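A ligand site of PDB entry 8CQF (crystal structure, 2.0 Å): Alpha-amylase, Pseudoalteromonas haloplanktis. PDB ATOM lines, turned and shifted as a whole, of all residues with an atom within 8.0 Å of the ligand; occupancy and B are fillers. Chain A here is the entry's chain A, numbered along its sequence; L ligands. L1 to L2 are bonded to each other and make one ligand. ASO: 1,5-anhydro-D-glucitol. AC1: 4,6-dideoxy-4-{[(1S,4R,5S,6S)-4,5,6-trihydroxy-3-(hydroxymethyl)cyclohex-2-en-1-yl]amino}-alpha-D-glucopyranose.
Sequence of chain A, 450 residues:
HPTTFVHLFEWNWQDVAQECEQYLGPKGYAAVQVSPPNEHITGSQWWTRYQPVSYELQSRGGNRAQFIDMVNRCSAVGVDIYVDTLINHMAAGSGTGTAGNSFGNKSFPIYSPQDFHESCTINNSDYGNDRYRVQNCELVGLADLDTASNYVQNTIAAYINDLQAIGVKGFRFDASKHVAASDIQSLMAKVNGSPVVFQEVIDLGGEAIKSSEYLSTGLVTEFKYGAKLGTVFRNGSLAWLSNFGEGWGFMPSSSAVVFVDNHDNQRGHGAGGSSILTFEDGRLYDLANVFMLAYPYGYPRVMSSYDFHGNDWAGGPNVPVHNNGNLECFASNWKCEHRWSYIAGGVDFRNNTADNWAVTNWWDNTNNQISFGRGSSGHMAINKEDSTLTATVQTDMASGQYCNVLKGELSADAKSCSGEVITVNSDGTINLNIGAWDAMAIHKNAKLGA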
ATOM      1  N   LYS A 106       6.697  13.421  10.767  1.00  0.00           N
ATOM      2  CA  LYS A 106       5.531  14.303  10.742  1.00  0.00           C
ATOM      3  C   LYS A 106       5.504  15.140   9.493  1.00  0.00           C
ATOM      4  O   LYS A 106       5.071  16.303   9.512  1.00  0.00           O
ATOM      5  CB  LYS A 106       5.482  15.243  11.939  1.00  0.00           C
ATOM      6  CG  LYS A 106       4.952  14.632  13.190  1.00  0.00           C
ATOM      7  CD  LYS A 106       4.912  15.674  14.266  1.00  0.00           C
ATOM      8  CE  LYS A 106       4.245  15.156  15.498  1.00  0.00           C
ATOM      9  NZ  LYS A 106       4.332  16.136  16.608  1.00  0.00           N
ATOM     10  N   SER A 107       6.013  14.592   8.396  1.00  0.00           N
ATOM     11  CA  SER A 107       5.878  15.206   7.089  1.00  0.00           C
ATOM     12  C   SER A 107       5.177  14.227   6.155  1.00  0.00           C
ATOM     13  O   SER A 107       5.637  13.093   5.965  1.00  0.00           O
ATOM     14  CB  SER A 107       7.240  15.631   6.534  1.00  0.00           C
ATOM     15  OG  SER A 107       7.041  16.537   5.462  1.00  0.00           O
ATOM     16  N   PHE A 108       4.103  14.687   5.538  1.00  0.00           N
ATOM     17  CA  PHE A 108       3.243  13.909   4.673  1.00  0.00           C
ATOM     18  C   PHE A 108       2.924  14.707   3.428  1.00  0.00           C
ATOM     19  O   PHE A 108       3.168  15.913   3.363  1.00  0.00           O
ATOM     20  CB  PHE A 108       1.940  13.547   5.415  1.00  0.00           C
ATOM     21  CG  PHE A 108       2.141  12.600   6.579  1.00  0.00           C
ATOM     22  CD1 PHE A 108       2.451  13.073   7.838  1.00  0.00           C
ATOM     23  CD2 PHE A 108       1.998  11.236   6.401  1.00  0.00           C
ATOM     24  CE1 PHE A 108       2.646  12.207   8.903  1.00  0.00           C
ATOM     25  CE2 PHE A 108       2.178  10.365   7.461  1.00  0.00           C
ATOM     26  CZ  PHE A 108       2.498  10.856   8.728  1.00  0.00           C
ATOM     27  N   PRO A 109       2.320  14.078   2.428  1.00  0.00           N
ATOM     28  CA  PRO A 109       1.959  14.832   1.220  1.00  0.00           C
ATOM     29  C   PRO A 109       1.127  16.082   1.474  1.00  0.00           C
ATOM     30  O   PRO A 109       1.198  17.028   0.663  1.00  0.00           O
ATOM     31  CB  PRO A 109       1.162  13.807   0.395  1.00  0.00           C
ATOM     32  CG  PRO A 109       1.685  12.481   0.839  1.00  0.00           C
ATOM     33  CD  PRO A 109       2.125  12.617   2.269  1.00  0.00           C
ATOM     34  N   ILE A 110       0.347  16.130   2.557  1.00  0.00           N
ATOM     35  CA  ILE A 110      -0.576  17.225   2.810  1.00  0.00           C
ATOM     36  C   ILE A 110      -0.399  17.815   4.192  1.00  0.00           C
ATOM     37  O   ILE A 110      -1.199  18.675   4.581  1.00  0.00           O
ATOM     38  CB  ILE A 110      -2.049  16.798   2.630  1.00  0.00           C
ATOM     39  CG1 ILE A 110      -2.346  15.757   3.724  1.00  0.00           C
ATOM     40  CG2 ILE A 110      -2.275  16.304   1.230  1.00  0.00           C
ATOM     41  CD1 ILE A 110      -3.483  14.892   3.448  1.00  0.00           C
ATOM     42  N   TYR A 111       0.563  17.340   4.975  1.00  0.00           N
ATOM     43  CA  TYR A 111       0.776  17.890   6.301  1.00  0.00           C
ATOM     44  C   TYR A 111       2.277  18.059   6.541  1.00  0.00           C
ATOM     45  O   TYR A 111       3.105  17.335   5.995  1.00  0.00           O
ATOM     46  CB  TYR A 111       0.212  16.996   7.417  1.00  0.00           C
ATOM     47  CG  TYR A 111      -1.302  16.870   7.471  1.00  0.00           C
ATOM     48  CD1 TYR A 111      -2.110  17.971   7.674  1.00  0.00           C
ATOM     49  CD2 TYR A 111      -1.912  15.615   7.362  1.00  0.00           C
ATOM     50  CE1 TYR A 111      -3.475  17.850   7.751  1.00  0.00           C
ATOM     51  CE2 TYR A 111      -3.256  15.486   7.441  1.00  0.00           C
ATOM     52  CZ  TYR A 111      -4.041  16.596   7.643  1.00  0.00           C
ATOM     53  OH  TYR A 111      -5.405  16.450   7.702  1.00  0.00           O
ATOM     54  N   SER A 112       2.597  19.005   7.415  1.00  0.00           N
ATOM     55  CA  SER A 112       3.951  19.259   7.892  1.00  0.00           C
ATOM     56  C   SER A 112       3.932  19.359   9.409  1.00  0.00           C
ATOM     57  O   SER A 112       2.868  19.333  10.033  1.00  0.00           O
ATOM     58  CB  SER A 112       4.488  20.546   7.252  1.00  0.00           C
ATOM     59  OG  SER A 112       3.596  21.640   7.470  1.00  0.00           O
ATOM     60  N   PRO A 113       5.102  19.429  10.045  1.00  0.00           N
ATOM     61  CA  PRO A 113       5.121  19.314  11.512  1.00  0.00           C
ATOM     62  C   PRO A 113       4.263  20.320  12.237  1.00  0.00           C
ATOM     63  O   PRO A 113       3.763  20.033  13.341  1.00  0.00           O
ATOM     64  CB  PRO A 113       6.613  19.514  11.850  1.00  0.00           C
ATOM     65  CG  PRO A 113       7.303  18.913  10.669  1.00  0.00           C
ATOM     66  CD  PRO A 113       6.428  19.187   9.454  1.00  0.00           C
ATOM     67  N   GLN A 114       4.061  21.498  11.661  1.00  0.00           N
ATOM     68  CA  GLN A 114       3.258  22.514  12.322  1.00  0.00           C
ATOM     69  C   GLN A 114       1.795  22.117  12.400  1.00  0.00           C
ATOM     70  O   GLN A 114       1.054  22.692  13.192  1.00  0.00           O
ATOM     71  CB  GLN A 114       3.409  23.851  11.577  1.00  0.00           C
ATOM     72  CG  GLN A 114       2.818  23.851  10.176  1.00  0.00           C
ATOM     73  CD  GLN A 114       3.153  25.111   9.381  1.00  0.00           C
ATOM     74  OE1 GLN A 114       2.904  26.235   9.811  1.00  0.00           O
ATOM     75  NE2 GLN A 114       3.722  24.916   8.213  1.00  0.00           N
ATOM     76  N   ASP A 115       1.369  21.155  11.595  1.00  0.00           N
ATOM     77  CA  ASP A 115      -0.023  20.740  11.588  1.00  0.00           C
ATOM     78  C   ASP A 115      -0.357  19.756  12.682  1.00  0.00           C
ATOM     79  O   ASP A 115      -1.491  19.264  12.729  1.00  0.00           O
ATOM     80  CB  ASP A 115      -0.369  20.154  10.235  1.00  0.00           C
ATOM     81  CG  ASP A 115      -0.298  21.165   9.146  1.00  0.00           C
ATOM     82  OD1 ASP A 115      -0.688  22.327   9.387  1.00  0.00           O
ATOM     83  OD2 ASP A 115       0.152  20.781   8.055  1.00  0.00           O
ATOM     84  N   PHE A 116       0.592  19.469  13.560  1.00  0.00           N
ATOM     85  CA  PHE A 116       0.418  18.482  14.614  1.00  0.00           C
ATOM     86  C   PHE A 116       0.598  19.106  15.992  1.00  0.00           C
ATOM     87  O   PHE A 116       1.275  20.117  16.165  1.00  0.00           O
ATOM     88  CB  PHE A 116       1.435  17.346  14.441  1.00  0.00           C
ATOM     89  CG  PHE A 116       1.245  16.561  13.169  1.00  0.00           C
ATOM     90  CD1 PHE A 116       1.817  16.981  12.010  1.00  0.00           C
ATOM     91  CD2 PHE A 116       0.456  15.418  13.159  1.00  0.00           C
ATOM     92  CE1 PHE A 116       1.656  16.304  10.839  1.00  0.00           C
ATOM     93  CE2 PHE A 116       0.280  14.711  11.964  1.00  0.00           C
ATOM     94  CZ  PHE A 116       0.870  15.152  10.808  1.00  0.00           C
ATOM     95  N   SER A 149      -6.814  23.376  14.254  1.00  0.00           N
ATOM     96  CA  SER A 149      -6.309  24.178  13.154  1.00  0.00           C
ATOM     97  C   SER A 149      -7.310  24.215  12.006  1.00  0.00           C
ATOM     98  O   SER A 149      -7.898  23.199  11.623  1.00  0.00           O
ATOM     99  CB  SER A 149      -4.978  23.598  12.672  1.00  0.00           C
ATOM    100  OG  SER A 149      -4.789  23.782  11.279  1.00  0.00           O
ATOM    101  N   ASN A 150      -7.475  25.400  11.427  1.00  0.00           N
ATOM    102  CA  ASN A 150      -8.395  25.532  10.310  1.00  0.00           C
ATOM    103  C   ASN A 150      -7.898  24.754   9.094  1.00  0.00           C
ATOM    104  O   ASN A 150      -8.693  24.171   8.351  1.00  0.00           O
ATOM    105  CB  ASN A 150      -8.585  26.998   9.952  1.00  0.00           C
ATOM    106  CG  ASN A 150      -9.837  27.223   9.170  1.00  0.00           C
ATOM    107  OD1 ASN A 150     -10.934  26.874   9.612  1.00  0.00           O
ATOM    108  ND2 ASN A 150      -9.687  27.775   7.978  1.00  0.00           N
ATOM    109  N   TYR A 151      -6.574  24.737   8.863  1.00  0.00           N
ATOM    110  CA  TYR A 151      -6.069  23.969   7.732  1.00  0.00           C
ATOM    111  C   TYR A 151      -6.381  22.484   7.900  1.00  0.00           C
ATOM    112  O   TYR A 151      -6.740  21.800   6.938  1.00  0.00           O
ATOM    113  CB  TYR A 151      -4.558  24.158   7.568  1.00  0.00           C
ATOM    114  CG  TYR A 151      -3.991  23.307   6.481  1.00  0.00           C
ATOM    115  CD1 TYR A 151      -4.247  23.592   5.158  1.00  0.00           C
ATOM    116  CD2 TYR A 151      -3.253  22.157   6.778  1.00  0.00           C
ATOM    117  CE1 TYR A 151      -3.759  22.775   4.143  1.00  0.00           C
ATOM    118  CE2 TYR A 151      -2.762  21.336   5.780  1.00  0.00           C
ATOM    119  CZ  TYR A 151      -3.020  21.647   4.476  1.00  0.00           C
ATOM    120  OH  TYR A 151      -2.527  20.843   3.475  1.00  0.00           O
ATOM    121  N   VAL A 152      -6.213  21.956   9.122  1.00  0.00           N
ATOM    122  CA  VAL A 152      -6.464  20.531   9.356  1.00  0.00           C
ATOM    123  C   VAL A 152      -7.943  20.226   9.177  1.00  0.00           C
ATOM    124  O   VAL A 152      -8.326  19.259   8.503  1.00  0.00           O
ATOM    125  CB  VAL A 152      -5.969  20.144  10.761  1.00  0.00           C
ATOM    126  CG1 VAL A 152      -6.469  18.759  11.163  1.00  0.00           C
ATOM    127  CG2 VAL A 152      -4.447  20.189  10.860  1.00  0.00           C
ATOM    128  N   THR A 155      -8.749  20.209   5.549  1.00  0.00           N
ATOM    129  CA  THR A 155      -8.225  19.051   4.830  1.00  0.00           C
ATOM    130  C   THR A 155      -9.047  17.784   5.117  1.00  0.00           C
ATOM    131  O   THR A 155      -9.378  17.016   4.210  1.00  0.00           O
ATOM    132  CB  THR A 155      -6.754  18.838   5.173  1.00  0.00           C
ATOM    133  OG1 THR A 155      -6.003  20.027   4.865  1.00  0.00           O
ATOM    134  CG2 THR A 155      -6.166  17.657   4.375  1.00  0.00           C
HETATM  135  C1  ASO L   1      -0.095  29.900   7.266  1.00  0.00           C
HETATM  136  C2  ASO L   1       0.476  28.921   8.290  1.00  0.00           C
HETATM  137  C3  ASO L   1       0.267  27.490   7.793  1.00  0.00           C
HETATM  138  C4  ASO L   1       0.161  27.490   6.275  1.00  0.00           C
HETATM  139  C5  ASO L   1       1.158  28.515   5.733  1.00  0.00           C
HETATM  140  C6  ASO L   1       1.202  28.484   4.229  1.00  0.00           C
HETATM  141  O2  ASO L   1       1.887  29.134   8.337  1.00  0.00           O
HETATM  142  O3  ASO L   1      -1.003  27.071   8.290  1.00  0.00           O
HETATM  143  O4  ASO L   1       0.655  26.220   5.815  1.00  0.00           O
HETATM  144  O5  ASO L   1       0.658  29.830   6.031  1.00  0.00           O
HETATM  145  O6  ASO L   1      -0.102  28.391   3.677  1.00  0.00           O
HETATM  146  C1  AC1 L   2      -0.395  25.267   5.609  1.00  0.00           C
HETATM  147  O2  AC1 L   2       0.326  24.080   7.545  1.00  0.00           O
HETATM  148  C2  AC1 L   2      -0.040  23.900   6.203  1.00  0.00           C
HETATM  149  C4A AC1 L   2       2.247  20.354   0.099  1.00  0.00           C
HETATM  150  C3  AC1 L   2       1.082  23.278   5.392  1.00  0.00           C
HETATM  151  O3  AC1 L   2       1.391  22.031   5.973  1.00  0.00           O
HETATM  152  C4  AC1 L   2       0.604  23.038   3.942  1.00  0.00           C
HETATM  153  N4A AC1 L   2       1.615  22.365   3.150  1.00  0.00           N
HETATM  154  C5  AC1 L   2       0.186  24.421   3.390  1.00  0.00           C
HETATM  155  O5  AC1 L   2      -0.758  25.068   4.255  1.00  0.00           O
HETATM  156  C6  AC1 L   2      -0.535  24.343   2.052  1.00  0.00           C
HETATM  157  C1B AC1 L   2       1.413  20.937   2.923  1.00  0.00           C
HETATM  158  C2B AC1 L   2       2.663  20.123   2.563  1.00  0.00           C
HETATM  159  O2B AC1 L   2       3.584  20.252   3.624  1.00  0.00           O
HETATM  160  C3B AC1 L   2       3.244  20.639   1.247  1.00  0.00           C
HETATM  161  O3B AC1 L   2       4.460  19.946   0.993  1.00  0.00           O
HETATM  162  O4  AC1 L   2       2.707  20.968  -1.094  1.00  0.00           O
HETATM  163  C5B AC1 L   2       0.833  20.696   0.474  1.00  0.00           C
HETATM  164  C7B AC1 L   2       0.465  20.779   1.758  1.00  0.00           C
HETATM  165  C6B AC1 L   2      -0.184  20.285  -0.569  1.00  0.00           C
HETATM  166  O6B AC1 L   2      -1.458  20.081   0.051  1.00  0.00           O
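The side-chain carboxylate of Asp 115 sits at hydrogen-bond distance from an oxygen (O3) of AC1 L2 (2.7 Å). The side-chain hydroxyl of Ser 112 lies within hydrogen-bond range of an oxygen (O3) of AC1 L2, 2.7 Å away. O2 of ASO L1 sits at hydrogen-bond distance from OE1 of Gln 114 (3.4 Å).
OG1 of Thr 155 sits at hydrogen-bond distance from O of Tyr 151. The backbone carbonyl oxygen (O) of Ile 110 sits at hydrogen-bond distance from the side-chain hydroxyl (OH) of Tyr 151, 2.8 Å away. The side-chain carboxylate (OD2) of Asp 115 is in hydrogen-bond range of the backbone NH (N) of Ser 112. The side-chain hydroxyl (OG) of Ser 112 lies within hydrogen-bond range of the side-chain amide nitrogen (NE2) of Gln 114 (3.4 Å). N of Tyr 151 is in hydrogen-bond range of OG of Ser 149, 3.2 Å away.
Merely in contact with the ligand: Tyr 151, Pro 109, Tyr 111 and Ile 110. Hydrophobic or aromatic side chains within 4 Å of the ligand: Tyr 151. The nearest printed residue that does not touch the ligand is Phe 108 (4.3 Å).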
